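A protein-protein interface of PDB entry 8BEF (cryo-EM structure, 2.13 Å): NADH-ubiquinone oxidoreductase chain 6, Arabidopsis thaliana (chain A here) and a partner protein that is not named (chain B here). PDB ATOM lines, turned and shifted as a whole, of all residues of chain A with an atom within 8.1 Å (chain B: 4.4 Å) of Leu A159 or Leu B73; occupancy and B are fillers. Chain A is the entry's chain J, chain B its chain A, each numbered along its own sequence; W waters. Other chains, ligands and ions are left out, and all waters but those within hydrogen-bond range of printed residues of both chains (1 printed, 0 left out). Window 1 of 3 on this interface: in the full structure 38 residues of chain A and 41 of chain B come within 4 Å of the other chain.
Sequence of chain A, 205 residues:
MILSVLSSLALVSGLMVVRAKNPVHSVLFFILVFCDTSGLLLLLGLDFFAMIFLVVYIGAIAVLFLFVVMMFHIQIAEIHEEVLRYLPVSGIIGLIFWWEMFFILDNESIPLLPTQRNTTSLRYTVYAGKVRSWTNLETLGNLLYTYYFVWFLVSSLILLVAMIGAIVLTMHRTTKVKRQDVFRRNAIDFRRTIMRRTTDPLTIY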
ATOM      1  N   ILE A  52      -8.559  18.824  -1.836  1.00  0.00           N
ATOM      2  CA  ILE A  52      -7.486  19.543  -1.165  1.00  0.00           C
ATOM      3  C   ILE A  52      -8.048  20.537  -0.162  1.00  0.00           C
ATOM      4  O   ILE A  52      -7.446  20.769   0.889  1.00  0.00           O
ATOM      5  CB  ILE A  52      -6.581  20.218  -2.213  1.00  0.00           C
ATOM      6  CG1 ILE A  52      -5.676  19.172  -2.858  1.00  0.00           C
ATOM      7  CG2 ILE A  52      -5.751  21.316  -1.599  1.00  0.00           C
ATOM      8  CD1 ILE A  52      -4.912  18.327  -1.865  1.00  0.00           C
ATOM      9  N   VAL A  55      -8.491  18.436   2.806  1.00  0.00           N
ATOM     10  CA  VAL A  55      -7.232  17.987   3.399  1.00  0.00           C
ATOM     11  C   VAL A  55      -6.533  19.127   4.135  1.00  0.00           C
ATOM     12  O   VAL A  55      -6.045  18.952   5.257  1.00  0.00           O
ATOM     13  CB  VAL A  55      -6.325  17.366   2.320  1.00  0.00           C
ATOM     14  CG1 VAL A  55      -4.894  17.251   2.821  1.00  0.00           C
ATOM     15  CG2 VAL A  55      -6.855  16.004   1.911  1.00  0.00           C
ATOM     16  N   VAL A  56      -6.483  20.308   3.528  1.00  0.00           N
ATOM     17  CA  VAL A  56      -5.676  21.408   4.050  1.00  0.00           C
ATOM     18  C   VAL A  56      -6.490  22.335   4.943  1.00  0.00           C
ATOM     19  O   VAL A  56      -6.081  22.642   6.065  1.00  0.00           O
ATOM     20  CB  VAL A  56      -5.022  22.185   2.885  1.00  0.00           C
ATOM     21  CG1 VAL A  56      -4.273  23.400   3.413  1.00  0.00           C
ATOM     22  CG2 VAL A  56      -4.092  21.278   2.095  1.00  0.00           C
ATOM     23  N   TYR A  57      -7.641  22.818   4.467  1.00  0.00           N
ATOM     24  CA  TYR A  57      -8.419  23.767   5.261  1.00  0.00           C
ATOM     25  C   TYR A  57      -9.015  23.098   6.492  1.00  0.00           C
ATOM     26  O   TYR A  57      -8.896  23.611   7.608  1.00  0.00           O
ATOM     27  CB  TYR A  57      -9.523  24.398   4.412  1.00  0.00           C
ATOM     28  CG  TYR A  57      -9.084  25.577   3.577  1.00  0.00           C
ATOM     29  CD1 TYR A  57      -8.471  26.679   4.159  1.00  0.00           C
ATOM     30  CD2 TYR A  57      -9.300  25.592   2.205  1.00  0.00           C
ATOM     31  CE1 TYR A  57      -8.077  27.758   3.395  1.00  0.00           C
ATOM     32  CE2 TYR A  57      -8.910  26.664   1.434  1.00  0.00           C
ATOM     33  CZ  TYR A  57      -8.303  27.746   2.035  1.00  0.00           C
ATOM     34  OH  TYR A  57      -7.912  28.811   1.266  1.00  0.00           O
ATOM     35  N   ALA A  60      -5.941  20.327   8.298  1.00  0.00           N
ATOM     36  CA  ALA A  60      -4.732  20.891   8.888  1.00  0.00           C
ATOM     37  C   ALA A  60      -4.946  22.256   9.524  1.00  0.00           C
ATOM     38  O   ALA A  60      -4.588  22.451  10.690  1.00  0.00           O
ATOM     39  CB  ALA A  60      -3.624  20.972   7.828  1.00  0.00           C
ATOM     40  N   ILE A  61      -5.545  23.202   8.799  1.00  0.00           N
ATOM     41  CA  ILE A  61      -5.662  24.568   9.304  1.00  0.00           C
ATOM     42  C   ILE A  61      -6.700  24.645  10.417  1.00  0.00           C
ATOM     43  O   ILE A  61      -6.443  25.197  11.496  1.00  0.00           O
ATOM     44  CB  ILE A  61      -5.991  25.532   8.149  1.00  0.00           C
ATOM     45  CG1 ILE A  61      -4.813  25.603   7.171  1.00  0.00           C
ATOM     46  CG2 ILE A  61      -6.360  26.910   8.686  1.00  0.00           C
ATOM     47  CD1 ILE A  61      -5.117  26.309   5.873  1.00  0.00           C
ATOM     48  N   TYR A 145       5.480  22.427 -11.965  1.00  0.00           N
ATOM     49  CA  TYR A 145       6.877  22.108 -11.717  1.00  0.00           C
ATOM     50  C   TYR A 145       7.807  22.457 -12.872  1.00  0.00           C
ATOM     51  O   TYR A 145       9.025  22.329 -12.718  1.00  0.00           O
ATOM     52  CB  TYR A 145       6.999  20.617 -11.383  1.00  0.00           C
ATOM     53  CG  TYR A 145       5.909  20.187 -10.435  1.00  0.00           C
ATOM     54  CD1 TYR A 145       5.956  20.533  -9.091  1.00  0.00           C
ATOM     55  CD2 TYR A 145       4.792  19.504 -10.898  1.00  0.00           C
ATOM     56  CE1 TYR A 145       4.944  20.167  -8.224  1.00  0.00           C
ATOM     57  CE2 TYR A 145       3.773  19.141 -10.044  1.00  0.00           C
ATOM     58  CZ  TYR A 145       3.854  19.471  -8.706  1.00  0.00           C
ATOM     59  OH  TYR A 145       2.841  19.104  -7.853  1.00  0.00           O
ATOM     60  N   PHE A 152       6.335  28.112  -7.401  1.00  0.00           N
ATOM     61  CA  PHE A 152       6.358  26.922  -6.554  1.00  0.00           C
ATOM     62  C   PHE A 152       7.464  27.010  -5.495  1.00  0.00           C
ATOM     63  O   PHE A 152       7.223  26.828  -4.290  1.00  0.00           O
ATOM     64  CB  PHE A 152       6.536  25.720  -7.494  1.00  0.00           C
ATOM     65  CG  PHE A 152       6.699  24.392  -6.825  1.00  0.00           C
ATOM     66  CD1 PHE A 152       5.779  23.932  -5.901  1.00  0.00           C
ATOM     67  CD2 PHE A 152       7.753  23.564  -7.184  1.00  0.00           C
ATOM     68  CE1 PHE A 152       5.932  22.691  -5.321  1.00  0.00           C
ATOM     69  CE2 PHE A 152       7.909  22.323  -6.603  1.00  0.00           C
ATOM     70  CZ  PHE A 152       6.998  21.887  -5.673  1.00  0.00           C
ATOM     71  N   LEU A 153       8.683  27.333  -5.929  1.00  0.00           N
ATOM     72  CA  LEU A 153       9.801  27.407  -4.990  1.00  0.00           C
ATOM     73  C   LEU A 153       9.654  28.578  -4.015  1.00  0.00           C
ATOM     74  O   LEU A 153      10.015  28.463  -2.834  1.00  0.00           O
ATOM     75  CB  LEU A 153      11.114  27.495  -5.763  1.00  0.00           C
ATOM     76  CG  LEU A 153      11.464  26.251  -6.583  1.00  0.00           C
ATOM     77  CD1 LEU A 153      12.831  26.395  -7.225  1.00  0.00           C
ATOM     78  CD2 LEU A 153      11.398  24.988  -5.721  1.00  0.00           C
ATOM     79  N   VAL A 154       9.130  29.713  -4.479  1.00  0.00           N
ATOM     80  CA  VAL A 154       8.900  30.832  -3.564  1.00  0.00           C
ATOM     81  C   VAL A 154       7.887  30.443  -2.489  1.00  0.00           C
ATOM     82  O   VAL A 154       8.020  30.823  -1.317  1.00  0.00           O
ATOM     83  CB  VAL A 154       8.460  32.089  -4.339  1.00  0.00           C
ATOM     84  CG1 VAL A 154       8.055  33.196  -3.373  1.00  0.00           C
ATOM     85  CG2 VAL A 154       9.586  32.573  -5.242  1.00  0.00           C
ATOM     86  N   SER A 155       6.866  29.671  -2.868  1.00  0.00           N
ATOM     87  CA  SER A 155       5.926  29.162  -1.872  1.00  0.00           C
ATOM     88  C   SER A 155       6.637  28.279  -0.850  1.00  0.00           C
ATOM     89  O   SER A 155       6.324  28.321   0.351  1.00  0.00           O
ATOM     90  CB  SER A 155       4.797  28.393  -2.556  1.00  0.00           C
ATOM     91  OG  SER A 155       5.159  27.041  -2.767  1.00  0.00           O
ATOM     92  N   SER A 156       7.588  27.460  -1.312  1.00  0.00           N
ATOM     93  CA  SER A 156       8.403  26.695  -0.368  1.00  0.00           C
ATOM     94  C   SER A 156       9.128  27.612   0.613  1.00  0.00           C
ATOM     95  O   SER A 156       9.213  27.315   1.813  1.00  0.00           O
ATOM     96  CB  SER A 156       9.415  25.822  -1.109  1.00  0.00           C
ATOM     97  OG  SER A 156      10.553  26.561  -1.501  1.00  0.00           O
ATOM     98  N   LEU A 157       9.668  28.726   0.118  1.00  0.00           N
ATOM     99  CA  LEU A 157      10.329  29.679   1.011  1.00  0.00           C
ATOM    100  C   LEU A 157       9.354  30.228   2.048  1.00  0.00           C
ATOM    101  O   LEU A 157       9.711  30.416   3.221  1.00  0.00           O
ATOM    102  CB  LEU A 157      10.951  30.819   0.205  1.00  0.00           C
ATOM    103  CG  LEU A 157      12.244  30.512  -0.550  1.00  0.00           C
ATOM    104  CD1 LEU A 157      12.795  31.779  -1.192  1.00  0.00           C
ATOM    105  CD2 LEU A 157      13.275  29.881   0.381  1.00  0.00           C
ATOM    106  N   ILE A 158       8.117  30.492   1.627  1.00  0.00           N
ATOM    107  CA  ILE A 158       7.091  30.977   2.548  1.00  0.00           C
ATOM    108  C   ILE A 158       6.843  29.956   3.661  1.00  0.00           C
ATOM    109  O   ILE A 158       6.757  30.306   4.849  1.00  0.00           O
ATOM    110  CB  ILE A 158       5.804  31.307   1.764  1.00  0.00           C
ATOM    111  CG1 ILE A 158       5.948  32.646   1.032  1.00  0.00           C
ATOM    112  CG2 ILE A 158       4.591  31.314   2.667  1.00  0.00           C
ATOM    113  CD1 ILE A 158       4.919  32.860  -0.060  1.00  0.00           C
ATOM    114  N   LEU A 159       6.755  28.677   3.294  1.00  0.00           N
ATOM    115  CA  LEU A 159       6.551  27.640   4.306  1.00  0.00           C
ATOM    116  C   LEU A 159       7.744  27.541   5.257  1.00  0.00           C
ATOM    117  O   LEU A 159       7.570  27.339   6.467  1.00  0.00           O
ATOM    118  CB  LEU A 159       6.275  26.293   3.641  1.00  0.00           C
ATOM    119  CG  LEU A 159       4.952  26.217   2.874  1.00  0.00           C
ATOM    120  CD1 LEU A 159       4.801  24.867   2.201  1.00  0.00           C
ATOM    121  CD2 LEU A 159       3.764  26.514   3.788  1.00  0.00           C
ATOM    122  N   LEU A 160       8.962  27.682   4.727  1.00  0.00           N
ATOM    123  CA  LEU A 160      10.146  27.676   5.584  1.00  0.00           C
ATOM    124  C   LEU A 160      10.092  28.811   6.601  1.00  0.00           C
ATOM    125  O   LEU A 160      10.436  28.623   7.779  1.00  0.00           O
ATOM    126  CB  LEU A 160      11.413  27.777   4.732  1.00  0.00           C
ATOM    127  CG  LEU A 160      12.738  27.928   5.487  1.00  0.00           C
ATOM    128  CD1 LEU A 160      13.002  26.710   6.336  1.00  0.00           C
ATOM    129  CD2 LEU A 160      13.893  28.165   4.525  1.00  0.00           C
ATOM    130  N   VAL A 161       9.668  29.998   6.158  1.00  0.00           N
ATOM    131  CA  VAL A 161       9.496  31.115   7.083  1.00  0.00           C
ATOM    132  C   VAL A 161       8.496  30.749   8.171  1.00  0.00           C
ATOM    133  O   VAL A 161       8.704  31.056   9.350  1.00  0.00           O
ATOM    134  CB  VAL A 161       9.066  32.388   6.328  1.00  0.00           C
ATOM    135  CG1 VAL A 161       8.647  33.472   7.314  1.00  0.00           C
ATOM    136  CG2 VAL A 161      10.191  32.885   5.445  1.00  0.00           C
ATOM    137  N   ALA A 162       7.390  30.103   7.792  1.00  0.00           N
ATOM    138  CA  ALA A 162       6.400  29.706   8.793  1.00  0.00           C
ATOM    139  C   ALA A 162       7.015  28.789   9.847  1.00  0.00           C
ATOM    140  O   ALA A 162       6.800  28.977  11.050  1.00  0.00           O
ATOM    141  CB  ALA A 162       5.206  29.025   8.123  1.00  0.00           C
ATOM    142  N   MET A 163       7.792  27.795   9.409  1.00  0.00           N
ATOM    143  CA  MET A 163       8.415  26.864  10.352  1.00  0.00           C
ATOM    144  C   MET A 163       9.357  27.592  11.308  1.00  0.00           C
ATOM    145  O   MET A 163       9.284  27.420  12.539  1.00  0.00           O
ATOM    146  CB  MET A 163       9.165  25.771   9.585  1.00  0.00           C
ATOM    147  CG  MET A 163       8.370  25.194   8.429  1.00  0.00           C
ATOM    148  SD  MET A 163       9.260  24.108   7.296  1.00  0.00           S
ATOM    149  CE  MET A 163       9.760  22.785   8.375  1.00  0.00           C
ATOM    150  N   ILE A 164      10.238  28.428  10.755  1.00  0.00           N
ATOM    151  CA  ILE A 164      11.204  29.147  11.582  1.00  0.00           C
ATOM    152  C   ILE A 164      10.486  30.041  12.583  1.00  0.00           C
ATOM    153  O   ILE A 164      10.826  30.068  13.772  1.00  0.00           O
ATOM    154  CB  ILE A 164      12.174  29.956  10.703  1.00  0.00           C
ATOM    155  CG1 ILE A 164      13.142  29.028   9.969  1.00  0.00           C
ATOM    156  CG2 ILE A 164      12.931  30.974  11.547  1.00  0.00           C
ATOM    157  CD1 ILE A 164      14.004  29.740   8.950  1.00  0.00           C
ATOM    158  N   GLY A 165       9.486  30.793  12.115  1.00  0.00           N
ATOM    159  CA  GLY A 165       8.769  31.697  12.999  1.00  0.00           C
ATOM    160  C   GLY A 165       8.037  30.971  14.110  1.00  0.00           C
ATOM    161  O   GLY A 165       8.066  31.399  15.268  1.00  0.00           O
ATOM    162  N   ALA A 166       7.380  29.856  13.774  1.00  0.00           N
ATOM    163  CA  ALA A 166       6.707  29.062  14.792  1.00  0.00           C
ATOM    164  C   ALA A 166       7.681  28.626  15.875  1.00  0.00           C
ATOM    165  O   ALA A 166       7.367  28.709  17.068  1.00  0.00           O
ATOM    166  CB  ALA A 166       6.033  27.846  14.159  1.00  0.00           C
ATOM    167  N   LEU B  69       0.756  20.679   9.411  1.00  0.00           N
ATOM    168  CA  LEU B  69       0.343  21.581   8.340  1.00  0.00           C
ATOM    169  C   LEU B  69       1.378  21.613   7.222  1.00  0.00           C
ATOM    170  O   LEU B  69       1.040  21.493   6.035  1.00  0.00           O
ATOM    171  CB  LEU B  69       0.121  22.979   8.911  1.00  0.00           C
ATOM    172  CG  LEU B  69      -0.207  24.100   7.930  1.00  0.00           C
ATOM    173  CD1 LEU B  69      -1.482  23.800   7.158  1.00  0.00           C
ATOM    174  CD2 LEU B  69      -0.313  25.401   8.688  1.00  0.00           C
ATOM    175  N   ILE B  70       2.654  21.753   7.594  1.00  0.00           N
ATOM    176  CA  ILE B  70       3.722  21.827   6.597  1.00  0.00           C
ATOM    177  C   ILE B  70       3.758  20.555   5.758  1.00  0.00           C
ATOM    178  O   ILE B  70       3.751  20.600   4.519  1.00  0.00           O
ATOM    179  CB  ILE B  70       5.079  22.086   7.277  1.00  0.00           C
ATOM    180  CG1 ILE B  70       5.070  23.397   8.073  1.00  0.00           C
ATOM    181  CG2 ILE B  70       6.205  22.069   6.248  1.00  0.00           C
ATOM    182  CD1 ILE B  70       4.404  24.555   7.382  1.00  0.00           C
ATOM    183  N   PHE B  71       3.776  19.394   6.416  1.00  0.00           N
ATOM    184  CA  PHE B  71       3.897  18.160   5.644  1.00  0.00           C
ATOM    185  C   PHE B  71       2.602  17.785   4.930  1.00  0.00           C
ATOM    186  O   PHE B  71       2.647  17.088   3.909  1.00  0.00           O
ATOM    187  CB  PHE B  71       4.391  17.031   6.538  1.00  0.00           C
ATOM    188  CG  PHE B  71       5.870  17.077   6.772  1.00  0.00           C
ATOM    189  CD1 PHE B  71       6.401  17.852   7.790  1.00  0.00           C
ATOM    190  CD2 PHE B  71       6.734  16.393   5.937  1.00  0.00           C
ATOM    191  CE1 PHE B  71       7.767  17.910   7.996  1.00  0.00           C
ATOM    192  CE2 PHE B  71       8.098  16.447   6.134  1.00  0.00           C
ATOM    193  CZ  PHE B  71       8.616  17.207   7.165  1.00  0.00           C
ATOM    194  N   ASP B  72       1.462  18.270   5.419  1.00  0.00           N
ATOM    195  CA  ASP B  72       0.209  18.168   4.686  1.00  0.00           C
ATOM    196  C   ASP B  72       0.307  18.890   3.350  1.00  0.00           C
ATOM    197  O   ASP B  72      -0.077  18.347   2.306  1.00  0.00           O
ATOM    198  CB  ASP B  72      -0.912  18.759   5.542  1.00  0.00           C
ATOM    199  CG  ASP B  72      -2.260  18.170   5.232  1.00  0.00           C
ATOM    200  OD1 ASP B  72      -2.431  16.947   5.396  1.00  0.00           O
ATOM    201  OD2 ASP B  72      -3.157  18.944   4.837  1.00  0.00           O
ATOM    202  N   LEU B  73       0.840  20.116   3.363  1.00  0.00           N
ATOM    203  CA  LEU B  73       1.039  20.814   2.096  1.00  0.00           C
ATOM    204  C   LEU B  73       2.076  20.115   1.225  1.00  0.00           C
ATOM    205  O   LEU B  73       1.966  20.141  -0.007  1.00  0.00           O
ATOM    206  CB  LEU B  73       1.446  22.267   2.324  1.00  0.00           C
ATOM    207  CG  LEU B  73       0.313  23.186   2.772  1.00  0.00           C
ATOM    208  CD1 LEU B  73       0.853  24.243   3.710  1.00  0.00           C
ATOM    209  CD2 LEU B  73      -0.422  23.796   1.585  1.00  0.00           C
ATOM    210  N   GLU B  74       3.086  19.495   1.839  1.00  0.00           N
ATOM    211  CA  GLU B  74       4.055  18.727   1.060  1.00  0.00           C
ATOM    212  C   GLU B  74       3.378  17.587   0.302  1.00  0.00           C
ATOM    213  O   GLU B  74       3.629  17.385  -0.892  1.00  0.00           O
ATOM    214  CB  GLU B  74       5.158  18.182   1.967  1.00  0.00           C
ATOM    215  CG  GLU B  74       6.486  17.985   1.263  1.00  0.00           C
ATOM    216  CD  GLU B  74       7.609  17.616   2.214  1.00  0.00           C
ATOM    217  OE1 GLU B  74       8.437  18.493   2.529  1.00  0.00           O
ATOM    218  OE2 GLU B  74       7.666  16.443   2.640  1.00  0.00           O
ATOM    219  N   VAL B  75       2.508  16.834   0.979  1.00  0.00           N
ATOM    220  CA  VAL B  75       1.772  15.760   0.309  1.00  0.00           C
ATOM    221  C   VAL B  75       0.866  16.331  -0.784  1.00  0.00           C
ATOM    222  O   VAL B  75       0.760  15.774  -1.895  1.00  0.00           O
ATOM    223  CB  VAL B  75       0.970  14.943   1.341  1.00  0.00           C
ATOM    224  CG1 VAL B  75       0.074  13.933   0.652  1.00  0.00           C
ATOM    225  CG2 VAL B  75       1.910  14.247   2.323  1.00  0.00           C
ATOM    226  N   THR B  76       0.190  17.442  -0.475  1.00  0.00           N
ATOM    227  CA  THR B  76      -0.645  18.127  -1.454  1.00  0.00           C
ATOM    228  C   THR B  76       0.127  18.407  -2.738  1.00  0.00           C
ATOM    229  O   THR B  76      -0.331  18.079  -3.837  1.00  0.00           O
ATOM    230  CB  THR B  76      -1.178  19.432  -0.855  1.00  0.00           C
ATOM    231  OG1 THR B  76      -2.092  19.138   0.208  1.00  0.00           O
ATOM    232  CG2 THR B  76      -1.872  20.279  -1.919  1.00  0.00           C
ATOM    233  N   PHE B  77       1.317  18.995  -2.610  1.00  0.00           N
ATOM    234  CA  PHE B  77       2.127  19.294  -3.785  1.00  0.00           C
ATOM    235  C   PHE B  77       2.718  18.040  -4.420  1.00  0.00           C
ATOM    236  O   PHE B  77       3.047  18.061  -5.608  1.00  0.00           O
ATOM    237  CB  PHE B  77       3.235  20.279  -3.418  1.00  0.00           C
ATOM    238  CG  PHE B  77       2.804  21.716  -3.470  1.00  0.00           C
ATOM    239  CD1 PHE B  77       2.608  22.348  -4.685  1.00  0.00           C
ATOM    240  CD2 PHE B  77       2.587  22.431  -2.306  1.00  0.00           C
ATOM    241  CE1 PHE B  77       2.209  23.669  -4.739  1.00  0.00           C
ATOM    242  CE2 PHE B  77       2.186  23.756  -2.353  1.00  0.00           C
ATOM    243  CZ  PHE B  77       1.998  24.374  -3.572  1.00  0.00           C
ATOM    244  N   LEU B 103      12.233  22.482   2.263  1.00  0.00           N
ATOM    245  CA  LEU B 103      11.392  22.017   3.366  1.00  0.00           C
ATOM    246  C   LEU B 103      12.176  21.134   4.338  1.00  0.00           C
ATOM    247  O   LEU B 103      11.940  21.168   5.548  1.00  0.00           O
ATOM    248  CB  LEU B 103      10.166  21.286   2.820  1.00  0.00           C
ATOM    249  CG  LEU B 103       9.142  22.189   2.119  1.00  0.00           C
ATOM    250  CD1 LEU B 103       7.781  21.517   2.021  1.00  0.00           C
ATOM    251  CD2 LEU B 103       9.026  23.542   2.806  1.00  0.00           C
HETATM  252  O   HOH W   1      -4.993  16.822   6.735  1.00  0.00           O
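Along chain A the printed residues that touch a printed residue of chain B span positions 52 to 163.
Printed residues of chain B that touch a printed residue of chain A: Leu B69, Ile B70, Asp B72, Leu B73, Thr B76, Phe B77 and Leu B103.
Hydrophobic or aromatic side chains of chain B that line the printed part of chain A: Leu B69, Ile B70, Leu B73, Phe B77 and Leu B103.
Among the printed residues, no Asp or Glu carboxylate lies within 4 Å of a Lys or Arg side-chain nitrogen of the other chain.
Printed residues of chain B within 4 Å of Leu A159: Leu B73 and Leu B103.
Of chain A, only Leu A159 comes within 4 Å of Leu B73.
Printed residues of chain B within 4 Å of Ile A61: Leu B69.
Of the printed residues of chain A, Leu B103 touches Ser A156 (3.9 Å), Leu A159 (3.98 Å) and Met A163 (3.9 Å).
Printed residues of chain B within 4 Å of Val A56: Asp B72 (3.6 Å) and Thr B76 (3.5 Å).
The nearest residue of chain B that does not touch Leu A159 is Ile B70 (4.1 Å).
The nearest residue of chain A that does not touch Leu B73 is Val A56 (4.3 Å).
The backbone carbonyl oxygen of Val A55 lies close to the side-chain carboxylate of Asp B72.
O of Phe B77 sits at hydrogen-bond distance from OH of Tyr A145.
The backbone carbonyl oxygen (O) of Asp B72 sits at hydrogen-bond distance from the side-chain hydroxyl (OG1) of Thr B76, at 3.0 Å.
O of Val A55 lies within hydrogen-bond range of N of Ala A60 (3.3 Å).
The backbone carbonyl oxygen (O) of Phe A152 is in hydrogen-bond range of the side-chain hydroxyl (OG) of Ser A155, at 2.6 Å.
N of Ile A61 lies within hydrogen-bond range of O of Val A56.
CD1 of Ile A52 touches OG1 of Thr B76 (3.6 Å).
Asp B72 touches Val A56 (OD2 to CA, 3.6 Å).
Val A56 touches Thr B76.
CB of Ala A60 touches CD1 of Leu B69, 3.6 Å away.
OD2 of Asp B72 touches CB of Ala A60, at 3.6 Å.
Ile A61 touches Leu B69 (CG1 to CD1, 3.8 Å).
Ser A156 touches Leu B103.
Leu A159 touches Leu B73.
CG1 of Ile B70 touches CG of Met A163, at 3.8 Å.
Met A163 touches Leu B103 (CE to O, 3.9 Å).
Water W1 bridges the backbone carbonyl oxygen (O) of Val A55 (2.8 Å) and the side-chain carboxylate (OD1) of Asp B72 (2.9 Å).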
